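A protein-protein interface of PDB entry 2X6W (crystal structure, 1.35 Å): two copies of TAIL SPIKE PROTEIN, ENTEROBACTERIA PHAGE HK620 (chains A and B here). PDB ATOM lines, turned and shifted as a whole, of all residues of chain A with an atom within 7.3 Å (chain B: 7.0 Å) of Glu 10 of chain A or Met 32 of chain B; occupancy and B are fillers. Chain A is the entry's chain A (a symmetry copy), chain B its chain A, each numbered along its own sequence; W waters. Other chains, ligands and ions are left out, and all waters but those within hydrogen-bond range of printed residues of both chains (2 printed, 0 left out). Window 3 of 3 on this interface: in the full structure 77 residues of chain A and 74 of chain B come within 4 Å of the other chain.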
ATOM      1  N   PHE A   5      -8.427 -32.707  26.883  1.00  0.00           N
ATOM      2  CA  PHE A   5      -7.041 -32.767  26.397  1.00  0.00           C
ATOM      3  C   PHE A   5      -6.606 -31.416  25.824  1.00  0.00           C
ATOM      4  O   PHE A   5      -5.483 -30.963  26.086  1.00  0.00           O
ATOM      5  CB  PHE A   5      -6.876 -33.870  25.335  1.00  0.00           C
ATOM      6  CG  PHE A   5      -5.437 -34.099  24.903  1.00  0.00           C
ATOM      7  CD1 PHE A   5      -4.455 -34.430  25.847  1.00  0.00           C
ATOM      8  CD2 PHE A   5      -5.068 -33.980  23.568  1.00  0.00           C
ATOM      9  CE1 PHE A   5      -3.133 -34.639  25.465  1.00  0.00           C
ATOM     10  CE2 PHE A   5      -3.746 -34.194  23.173  1.00  0.00           C
ATOM     11  CZ  PHE A   5      -2.778 -34.526  24.130  1.00  0.00           C
ATOM     12  N   ARG A   6      -7.482 -30.786  25.036  1.00  0.00           N
ATOM     13  CA  ARG A   6      -7.218 -29.461  24.463  1.00  0.00           C
ATOM     14  C   ARG A   6      -6.890 -28.456  25.574  1.00  0.00           C
ATOM     15  O   ARG A   6      -5.972 -27.635  25.432  1.00  0.00           O
ATOM     16  CB  ARG A   6      -8.415 -28.979  23.620  1.00  0.00           C
ATOM     17  CG  ARG A   6      -8.281 -27.539  23.070  1.00  0.00           C
ATOM     18  CD  ARG A   6      -9.633 -26.886  22.717  1.00  0.00           C
ATOM     19  NE  ARG A   6      -9.842 -26.733  21.274  1.00  0.00           N
ATOM     20  CZ  ARG A   6      -9.282 -25.786  20.509  1.00  0.00           C
ATOM     21  NH1 ARG A   6      -8.443 -24.896  21.035  1.00  0.00           N
ATOM     22  NH2 ARG A   6      -9.548 -25.735  19.200  1.00  0.00           N
ATOM     23  N   ALA A   7      -7.634 -28.539  26.676  1.00  0.00           N
ATOM     24  CA  ALA A   7      -7.421 -27.695  27.840  1.00  0.00           C
ATOM     25  C   ALA A   7      -6.005 -27.863  28.391  1.00  0.00           C
ATOM     26  O   ALA A   7      -5.315 -26.874  28.629  1.00  0.00           O
ATOM     27  CB  ALA A   7      -8.450 -28.019  28.924  1.00  0.00           C
ATOM     28  N   ILE A   8      -5.581 -29.112  28.588  1.00  0.00           N
ATOM     29  CA  ILE A   8      -4.230 -29.409  29.082  1.00  0.00           C
ATOM     30  C   ILE A   8      -3.166 -28.853  28.114  1.00  0.00           C
ATOM     31  O   ILE A   8      -2.247 -28.164  28.550  1.00  0.00           O
ATOM     32  CB  ILE A   8      -4.020 -30.940  29.324  1.00  0.00           C
ATOM     33  CG1 ILE A   8      -4.804 -31.392  30.571  1.00  0.00           C
ATOM     34  CG2 ILE A   8      -2.536 -31.281  29.466  1.00  0.00           C
ATOM     35  CD1 ILE A   8      -4.941 -32.927  30.718  1.00  0.00           C
ATOM     36  N   ILE A   9      -3.332 -29.097  26.814  1.00  0.00           N
ATOM     37  CA  ILE A   9      -2.315 -28.718  25.806  1.00  0.00           C
ATOM     38  C   ILE A   9      -2.169 -27.196  25.655  1.00  0.00           C
ATOM     39  O   ILE A   9      -1.063 -26.689  25.471  1.00  0.00           O
ATOM     40  CB  ILE A   9      -2.618 -29.370  24.427  1.00  0.00           C
ATOM     41  CG1 ILE A   9      -2.439 -30.900  24.494  1.00  0.00           C
ATOM     42  CG2 ILE A   9      -1.723 -28.781  23.318  1.00  0.00           C
ATOM     43  CD1 ILE A   9      -0.992 -31.383  24.638  1.00  0.00           C
ATOM     44  N   GLU A  10      -3.270 -26.463  25.758  1.00  0.00           N
ATOM     45  CA  GLU A  10      -3.228 -24.999  25.684  1.00  0.00           C
ATOM     46  C   GLU A  10      -2.825 -24.306  27.003  1.00  0.00           C
ATOM     47  O   GLU A  10      -2.512 -23.100  27.005  1.00  0.00           O
ATOM     48  CB  GLU A  10      -4.572 -24.469  25.142  1.00  0.00           C
ATOM     49  CG  GLU A  10      -4.816 -24.855  23.673  1.00  0.00           C
ATOM     50  CD  GLU A  10      -5.908 -24.039  22.999  1.00  0.00           C
ATOM     51  OE1 GLU A  10      -7.083 -24.205  23.392  1.00  0.00           O
ATOM     52  OE2 GLU A  10      -5.593 -23.249  22.062  1.00  0.00           O
ATOM     53  N   SER A  11      -2.815 -25.070  28.097  1.00  0.00           N
ATOM     54  CA  SER A  11      -2.408 -24.569  29.419  1.00  0.00           C
ATOM     55  C   SER A  11      -0.893 -24.461  29.530  1.00  0.00           C
ATOM     56  O   SER A  11      -0.175 -25.023  28.708  1.00  0.00           O
ATOM     57  CB  SER A  11      -2.924 -25.481  30.545  1.00  0.00           C
ATOM     58  OG  SER A  11      -2.158 -26.673  30.680  1.00  0.00           O
ATOM     59  N   PRO A  12      -0.401 -23.783  30.592  1.00  0.00           N
ATOM     60  CA  PRO A  12       1.057 -23.723  30.784  1.00  0.00           C
ATOM     61  C   PRO A  12       1.758 -25.083  30.979  1.00  0.00           C
ATOM     62  O   PRO A  12       2.977 -25.179  30.791  1.00  0.00           O
ATOM     63  CB  PRO A  12       1.213 -22.859  32.042  1.00  0.00           C
ATOM     64  CG  PRO A  12      -0.006 -22.040  32.088  1.00  0.00           C
ATOM     65  CD  PRO A  12      -1.103 -22.890  31.535  1.00  0.00           C
ATOM     66  N   GLU A  13       0.998 -26.119  31.322  1.00  0.00           N
ATOM     67  CA  GLU A  13       1.534 -27.470  31.443  1.00  0.00           C
ATOM     68  C   GLU A  13       1.464 -28.283  30.137  1.00  0.00           C
ATOM     69  O   GLU A  13       1.847 -29.450  30.123  1.00  0.00           O
ATOM     70  CB  GLU A  13       0.809 -28.228  32.563  1.00  0.00           C
ATOM     71  CG  GLU A  13       1.040 -27.656  33.952  1.00  0.00           C
ATOM     72  CD  GLU A  13       0.622 -28.626  35.041  1.00  0.00           C
ATOM     73  OE1 GLU A  13      -0.420 -29.295  34.871  1.00  0.00           O
ATOM     74  OE2 GLU A  13       1.336 -28.726  36.060  1.00  0.00           O
ATOM     75  N   GLY A  14       0.985 -27.676  29.054  1.00  0.00           N
ATOM     76  CA  GLY A  14       0.799 -28.393  27.786  1.00  0.00           C
ATOM     77  C   GLY A  14       2.036 -29.068  27.221  1.00  0.00           C
ATOM     78  O   GLY A  14       1.997 -30.246  26.872  1.00  0.00           O
ATOM     79  N   ALA A  15       3.164 -28.351  27.202  1.00  0.00           N
ATOM     80  CA  ALA A  15       4.431 -28.908  26.722  1.00  0.00           C
ATOM     81  C   ALA A  15       4.876 -30.107  27.573  1.00  0.00           C
ATOM     82  O   ALA A  15       5.633 -30.982  27.104  1.00  0.00           O
ATOM     83  CB  ALA A  15       5.511 -27.829  26.701  1.00  0.00           C
ATOM     84  N   LEU A  37      12.913 -28.033  26.807  1.00  0.00           N
ATOM     85  CA  LEU A  37      12.918 -26.569  26.921  1.00  0.00           C
ATOM     86  C   LEU A  37      13.522 -26.106  28.252  1.00  0.00           C
ATOM     87  O   LEU A  37      14.181 -25.083  28.299  1.00  0.00           O
ATOM     88  CB  LEU A  37      11.513 -25.998  26.748  1.00  0.00           C
ATOM     89  CG  LEU A  37      10.830 -26.329  25.413  1.00  0.00           C
ATOM     90  CD1 LEU A  37       9.445 -25.705  25.438  1.00  0.00           C
ATOM     91  CD2 LEU A  37      11.624 -25.837  24.181  1.00  0.00           C
ATOM     92  N   PHE B   5      -8.962 -28.588  16.420  1.00  0.00           N
ATOM     93  CA  PHE B   5      -7.755 -28.445  17.247  1.00  0.00           C
ATOM     94  C   PHE B   5      -6.587 -29.231  16.645  1.00  0.00           C
ATOM     95  O   PHE B   5      -5.456 -28.727  16.603  1.00  0.00           O
ATOM     96  CB  PHE B   5      -8.018 -28.910  18.692  1.00  0.00           C
ATOM     97  CG  PHE B   5      -6.864 -28.642  19.643  1.00  0.00           C
ATOM     98  CD1 PHE B   5      -6.377 -27.340  19.822  1.00  0.00           C
ATOM     99  CD2 PHE B   5      -6.269 -29.681  20.350  1.00  0.00           C
ATOM    100  CE1 PHE B   5      -5.319 -27.081  20.690  1.00  0.00           C
ATOM    101  CE2 PHE B   5      -5.212 -29.431  21.228  1.00  0.00           C
ATOM    102  CZ  PHE B   5      -4.739 -28.123  21.395  1.00  0.00           C
ATOM    103  N   ILE B   8      -4.987 -27.262  13.895  1.00  0.00           N
ATOM    104  CA  ILE B   8      -4.098 -26.213  14.412  1.00  0.00           C
ATOM    105  C   ILE B   8      -2.756 -26.819  14.870  1.00  0.00           C
ATOM    106  O   ILE B   8      -1.701 -26.326  14.478  1.00  0.00           O
ATOM    107  CB  ILE B   8      -4.767 -25.399  15.568  1.00  0.00           C
ATOM    108  CG1 ILE B   8      -5.868 -24.481  15.001  1.00  0.00           C
ATOM    109  CG2 ILE B   8      -3.731 -24.584  16.344  1.00  0.00           C
ATOM    110  CD1 ILE B   8      -6.812 -23.880  16.071  1.00  0.00           C
ATOM    111  N   ILE B   9      -2.804 -27.911  15.633  1.00  0.00           N
ATOM    112  CA  ILE B   9      -1.587 -28.509  16.229  1.00  0.00           C
ATOM    113  C   ILE B   9      -0.642 -29.104  15.175  1.00  0.00           C
ATOM    114  O   ILE B   9       0.578 -29.007  15.303  1.00  0.00           O
ATOM    115  CB  ILE B   9      -1.951 -29.581  17.296  1.00  0.00           C
ATOM    116  CG1 ILE B   9      -2.615 -28.928  18.524  1.00  0.00           C
ATOM    117  CG2 ILE B   9      -0.709 -30.385  17.731  1.00  0.00           C
ATOM    118  CD1 ILE B   9      -1.685 -28.077  19.396  1.00  0.00           C
ATOM    119  N   GLY B  14       1.168 -24.809  15.114  1.00  0.00           N
ATOM    120  CA  GLY B  14       0.849 -25.718  16.222  1.00  0.00           C
ATOM    121  C   GLY B  14       1.623 -25.489  17.509  1.00  0.00           C
ATOM    122  O   GLY B  14       1.030 -25.397  18.582  1.00  0.00           O
ATOM    123  N   ALA B  15       2.944 -25.314  17.400  1.00  0.00           N
ATOM    124  CA  ALA B  15       3.789 -25.041  18.564  1.00  0.00           C
ATOM    125  C   ALA B  15       3.389 -23.728  19.254  1.00  0.00           C
ATOM    126  O   ALA B  15       3.641 -23.535  20.461  1.00  0.00           O
ATOM    127  CB  ALA B  15       5.261 -25.011  18.156  1.00  0.00           C
ATOM    128  N   GLY B  16       2.785 -22.824  18.477  1.00  0.00           N
ATOM    129  CA  GLY B  16       2.239 -21.572  18.998  1.00  0.00           C
ATOM    130  C   GLY B  16       0.955 -21.714  19.802  1.00  0.00           C
ATOM    131  O   GLY B  16       0.413 -20.712  20.271  1.00  0.00           O
ATOM    132  N   HIS B  17       0.453 -22.946  19.932  1.00  0.00           N
ATOM    133  CA  HIS B  17      -0.750 -23.226  20.725  1.00  0.00           C
ATOM    134  C   HIS B  17      -0.485 -24.197  21.877  1.00  0.00           C
ATOM    135  O   HIS B  17      -1.417 -24.566  22.584  1.00  0.00           O
ATOM    136  CB  HIS B  17      -1.870 -23.767  19.819  1.00  0.00           C
ATOM    137  CG  HIS B  17      -2.378 -22.758  18.843  1.00  0.00           C
ATOM    138  ND1 HIS B  17      -1.679 -22.398  17.712  1.00  0.00           N
ATOM    139  CD2 HIS B  17      -3.499 -21.998  18.852  1.00  0.00           C
ATOM    140  CE1 HIS B  17      -2.358 -21.472  17.053  1.00  0.00           C
ATOM    141  NE2 HIS B  17      -3.462 -21.205  17.731  1.00  0.00           N
ATOM    142  N   VAL B  18       0.769 -24.621  22.067  1.00  0.00           N
ATOM    143  CA  VAL B  18       1.120 -25.536  23.169  1.00  0.00           C
ATOM    144  C   VAL B  18       1.789 -24.743  24.280  1.00  0.00           C
ATOM    145  O   VAL B  18       2.864 -24.195  24.078  1.00  0.00           O
ATOM    146  CB  VAL B  18       2.077 -26.658  22.706  1.00  0.00           C
ATOM    147  CG1 VAL B  18       2.414 -27.587  23.867  1.00  0.00           C
ATOM    148  CG2 VAL B  18       1.440 -27.447  21.557  1.00  0.00           C
ATOM    149  N   GLY B  19       1.165 -24.687  25.453  1.00  0.00           N
ATOM    150  CA  GLY B  19       1.627 -23.788  26.500  1.00  0.00           C
ATOM    151  C   GLY B  19       2.849 -24.322  27.217  1.00  0.00           C
ATOM    152  O   GLY B  19       3.087 -25.540  27.278  1.00  0.00           O
ATOM    153  N   TYR B  20       3.638 -23.395  27.742  1.00  0.00           N
ATOM    154  CA  TYR B  20       4.844 -23.744  28.480  1.00  0.00           C
ATOM    155  C   TYR B  20       5.115 -22.718  29.550  1.00  0.00           C
ATOM    156  O   TYR B  20       4.968 -21.520  29.322  1.00  0.00           O
ATOM    157  CB  TYR B  20       6.044 -23.805  27.539  1.00  0.00           C
ATOM    158  CG  TYR B  20       7.411 -23.903  28.199  1.00  0.00           C
ATOM    159  CD1 TYR B  20       7.861 -25.106  28.752  1.00  0.00           C
ATOM    160  CD2 TYR B  20       8.268 -22.800  28.228  1.00  0.00           C
ATOM    161  CE1 TYR B  20       9.113 -25.205  29.327  1.00  0.00           C
ATOM    162  CE2 TYR B  20       9.536 -22.885  28.806  1.00  0.00           C
ATOM    163  CZ  TYR B  20       9.952 -24.087  29.351  1.00  0.00           C
ATOM    164  OH  TYR B  20      11.203 -24.181  29.899  1.00  0.00           O
ATOM    165  N   GLN B  21       5.570 -23.193  30.704  1.00  0.00           N
ATOM    166  CA  GLN B  21       6.047 -22.322  31.767  1.00  0.00           C
ATOM    167  C   GLN B  21       7.291 -22.979  32.361  1.00  0.00           C
ATOM    168  O   GLN B  21       7.246 -24.128  32.774  1.00  0.00           O
ATOM    169  CB  GLN B  21       4.943 -22.133  32.810  1.00  0.00           C
ATOM    170  CG  GLN B  21       5.275 -21.264  33.968  1.00  0.00           C
ATOM    171  CD  GLN B  21       4.063 -21.047  34.864  1.00  0.00           C
ATOM    172  OE1 GLN B  21       3.492 -22.005  35.407  1.00  0.00           O
ATOM    173  NE2 GLN B  21       3.684 -19.789  35.039  1.00  0.00           N
ATOM    174  N   THR B  29       6.959 -16.789  33.088  1.00  0.00           N
ATOM    175  CA  THR B  29       6.110 -16.403  31.996  1.00  0.00           C
ATOM    176  C   THR B  29       5.327 -17.585  31.455  1.00  0.00           C
ATOM    177  O   THR B  29       5.873 -18.689  31.275  1.00  0.00           O
ATOM    178  CB  THR B  29       6.974 -15.778  30.869  1.00  0.00           C
ATOM    179  OG1 THR B  29       7.825 -14.770  31.441  1.00  0.00           O
ATOM    180  CG2 THR B  29       6.105 -15.174  29.753  1.00  0.00           C
ATOM    181  N   MET B  30       4.041 -17.343  31.193  1.00  0.00           N
ATOM    182  CA  MET B  30       3.215 -18.313  30.493  1.00  0.00           C
ATOM    183  C   MET B  30       3.425 -18.101  29.019  1.00  0.00           C
ATOM    184  O   MET B  30       2.911 -17.126  28.433  1.00  0.00           O
ATOM    185  CB  MET B  30       1.740 -18.133  30.875  1.00  0.00           C
ATOM    186  CG  MET B  30       1.521 -18.367  32.340  1.00  0.00           C
ATOM    187  SD  MET B  30      -0.192 -18.168  32.822  1.00  0.00           S
ATOM    188  CE  MET B  30      -0.035 -18.660  34.537  1.00  0.00           C
ATOM    189  N   ARG B  31       4.216 -18.997  28.428  1.00  0.00           N
ATOM    190  CA  ARG B  31       4.647 -18.880  27.039  1.00  0.00           C
ATOM    191  C   ARG B  31       4.014 -19.996  26.215  1.00  0.00           C
ATOM    192  O   ARG B  31       3.237 -20.812  26.737  1.00  0.00           O
ATOM    193  CB  ARG B  31       6.188 -18.977  26.967  1.00  0.00           C
ATOM    194  CG  ARG B  31       6.929 -18.034  27.932  1.00  0.00           C
ATOM    195  CD  ARG B  31       8.429 -18.199  27.793  1.00  0.00           C
ATOM    196  NE  ARG B  31       8.967 -17.584  26.585  1.00  0.00           N
ATOM    197  CZ  ARG B  31      10.237 -17.707  26.209  1.00  0.00           C
ATOM    198  NH1 ARG B  31      11.066 -18.446  26.939  1.00  0.00           N
ATOM    199  NH2 ARG B  31      10.670 -17.107  25.112  1.00  0.00           N
ATOM    200  N   MET B  32       4.304 -19.981  24.920  1.00  0.00           N
ATOM    201  CA  MET B  32       4.037 -21.114  24.033  1.00  0.00           C
ATOM    202  C   MET B  32       5.359 -21.733  23.597  1.00  0.00           C
ATOM    203  O   MET B  32       6.404 -21.062  23.594  1.00  0.00           O
ATOM    204  CB  MET B  32       3.221 -20.657  22.827  1.00  0.00           C
ATOM    205  CG  MET B  32       1.871 -20.087  23.220  1.00  0.00           C
ATOM    206  SD  MET B  32       0.728 -21.376  23.765  1.00  0.00           S
ATOM    207  CE  MET B  32      -0.246 -20.513  24.992  1.00  0.00           C
ATOM    208  N   VAL B  33       5.328 -23.015  23.241  1.00  0.00           N
ATOM    209  CA  VAL B  33       6.527 -23.719  22.792  1.00  0.00           C
ATOM    210  C   VAL B  33       7.246 -22.971  21.662  1.00  0.00           C
ATOM    211  O   VAL B  33       8.476 -22.847  21.699  1.00  0.00           O
ATOM    212  CB  VAL B  33       6.193 -25.149  22.333  1.00  0.00           C
ATOM    213  CG1 VAL B  33       7.376 -25.757  21.577  1.00  0.00           C
ATOM    214  CG2 VAL B  33       5.797 -26.022  23.545  1.00  0.00           C
ATOM    215  N   SER B  34       6.499 -22.446  20.686  1.00  0.00           N
ATOM    216  CA  SER B  34       7.096 -21.705  19.570  1.00  0.00           C
ATOM    217  C   SER B  34       7.957 -20.529  20.082  1.00  0.00           C
ATOM    218  O   SER B  34       8.985 -20.248  19.504  1.00  0.00           O
ATOM    219  CB  SER B  34       6.017 -21.191  18.611  1.00  0.00           C
ATOM    220  OG  SER B  34       5.151 -20.287  19.274  1.00  0.00           O
ATOM    221  N   ASP B  35       7.527 -19.855  21.161  1.00  0.00           N
ATOM    222  CA  ASP B  35       8.291 -18.730  21.732  1.00  0.00           C
ATOM    223  C   ASP B  35       9.681 -19.159  22.175  1.00  0.00           C
ATOM    224  O   ASP B  35      10.681 -18.454  21.967  1.00  0.00           O
ATOM    225  CB  ASP B  35       7.572 -18.094  22.929  1.00  0.00           C
ATOM    226  CG  ASP B  35       6.232 -17.523  22.566  1.00  0.00           C
ATOM    227  OD1 ASP B  35       6.145 -16.802  21.545  1.00  0.00           O
ATOM    228  OD2 ASP B  35       5.271 -17.766  23.324  1.00  0.00           O
ATOM    229  N   VAL B  36       9.747 -20.316  22.811  1.00  0.00           N
ATOM    230  CA  VAL B  36      11.033 -20.818  23.295  1.00  0.00           C
ATOM    231  C   VAL B  36      11.901 -21.273  22.118  1.00  0.00           C
ATOM    232  O   VAL B  36      13.084 -20.952  22.046  1.00  0.00           O
ATOM    233  CB  VAL B  36      10.858 -21.962  24.304  1.00  0.00           C
ATOM    234  CG1 VAL B  36      12.230 -22.365  24.887  1.00  0.00           C
ATOM    235  CG2 VAL B  36       9.877 -21.559  25.428  1.00  0.00           C
ATOM    236  N   LEU B  37      11.313 -21.976  21.156  1.00  0.00           N
ATOM    237  CA  LEU B  37      12.067 -22.381  19.962  1.00  0.00           C
ATOM    238  C   LEU B  37      12.590 -21.167  19.184  1.00  0.00           C
ATOM    239  O   LEU B  37      13.669 -21.223  18.622  1.00  0.00           O
ATOM    240  CB  LEU B  37      11.222 -23.270  19.054  1.00  0.00           C
ATOM    241  CG  LEU B  37      10.703 -24.563  19.698  1.00  0.00           C
ATOM    242  CD1 LEU B  37       9.870 -25.294  18.660  1.00  0.00           C
ATOM    243  CD2 LEU B  37      11.831 -25.477  20.230  1.00  0.00           C
HETATM  244  O   HOH W   1       4.444 -25.852  33.415  1.00  0.00           O
HETATM  245  O   HOH W   2      -3.009 -22.048  22.886  1.00  0.00           O
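N of Val 33 of chain B is in hydrogen-bond range of O of Val 18 of chain B (2.9 Å). N of Glu 13 of chain A sits close to OG of Ser 11 of chain A, at 3.3 Å. The backbone NH of Val 33 of chain B lies within hydrogen-bond range of the backbone carbonyl oxygen of Ala 15 of chain B (3.3 Å). The side-chain hydroxyl of Ser 11 of chain A sits at hydrogen-bond distance from the backbone carbonyl oxygen of Ile 8 of chain A, 2.6 Å away. The backbone NH (N) of Gly 19 of chain B sits at hydrogen-bond distance from the side-chain sulfur (SD) of Met 32 of chain B, 3.7 Å away. The guanidinium group of Arg 6 of chain A lies within salt-bridge range of the side-chain carboxylate of Glu 10 of chain A, 2.8 Å away.
Phe 5 of chain B touches Ile 9 of chain A (CZ to CG2, 3.6 Å). Ile 9 of chain B touches Ile 9 of chain A (CD1 to CG2, 3.98 Å). Gly 19 of chain B touches Ser 11 of chain A. Gly 19 of chain B touches Pro 12 of chain A (O to O, 3.5 Å). SD of Met 30 of chain B touches CG of Pro 12 of chain A, at 3.9 Å. C of Gly 14 of chain A touches CG1 of Val 18 of chain B, 3.7 Å away. Ala 15 of chain A touches Val 18 of chain B. CB of Ala 15 of chain A touches CG2 of Val 33 of chain B, 3.6 Å away. Leu 37 of chain A touches Val 36 of chain B (CD2 to CG1, 3.6 Å). CD2 of Leu 37 of chain B touches CD2 of Leu 37 of chain A, 3.97 Å away.
Of the 20 printed residues of chain B, 12 touch a printed residue of chain A. Printed residues of chain B that touch a printed residue of chain A: Phe 5, Ile 9, His 17, Val 18, Gly 19, Tyr 20, Gln 21, Met 30, Met 32, Val 33, Val 36 and Leu 37. Hydrophobic or aromatic side chains of chain B within 4 Å of the printed part of chain A: Phe 5, Ile 9, Val 18, Tyr 20, Met 30, Met 32, Val 33, Val 36 and Leu 37. Along chain A the printed residues that touch a printed residue of chain B span positions 6 to 37.
Water W2 bridges OE2 of Glu 10 of chain A (3.0 Å) and O of His 17 of chain B (3.0 Å). Water W1 bridges O of Pro 12 of chain A (3.1 Å) and O of Gln 21 of chain B (3.4 Å).
Printed residues of chain B within 4 Å of Glu 10 of chain A: Phe 5 (3.8 Å), His 17 (3.6 Å) and Met 32 (3.98 Å). Of the printed residues of chain A, Met 32 of chain B touches Glu 10. Printed residues of chain B within 4 Å of Ser 11 of chain A: Gly 19 (3.1 Å). Of the printed residues of chain B, Gly 14 of chain A touches Val 18 (3.7 Å) and Gly 19 (3.5 Å). Of the printed residues of chain A, Gln 21 of chain B touches Pro 12. Of the printed residues of chain A, Phe 5 of chain B touches Arg 6 (3.4 Å), Ile 9 (3.6 Å) and Glu 10 (3.8 Å). Phe 5 of chain A touches none of the printed residues of chain B. The nearest printed residue of chain B that does not touch Glu 10 of chain A is Gly 19 of chain B (4.2 Å). The nearest printed residue of chain B that does not touch Arg 6 of chain A is Ile 8 of chain B (4.6 Å).
Ile 9 of chain A touches Phe 5 of chain B, but with the chains exchanged Phe 5 of chain A does not touch Ile 9 of chain B (7.1 Å). Ile 9 of chain A touches its own counterpart, Ile 9 of chain B. Leu 37 of chain A touches its own counterpart, Leu 37 of chain B. Positions printed for both chains: 5, 8, 9, 14, 15 and 37. Of the 22 pairs that touch across the chains among the printed residues, 2 have their exchanged pair printed and touching as well.
N of Gln 21 of chain B sits at hydrogen-bond distance from O of Pro 12 of chain A. OH of Tyr 20 of chain B sits close to O of Leu 37 of chain A (3.5 Å). The backbone carbonyl oxygen of Gly 19 of chain B is in hydrogen-bond range of the backbone NH of Gly 14 of chain A. The backbone carbonyl oxygen (O) of Gly 19 of chain B lies within hydrogen-bond range of the backbone NH (N) of Ala 15 of chain A (2.8 Å). The backbone NH (N) of Gly 19 of chain B lies within hydrogen-bond range of the backbone carbonyl oxygen (O) of Ile 9 of chain A (3.0 Å).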
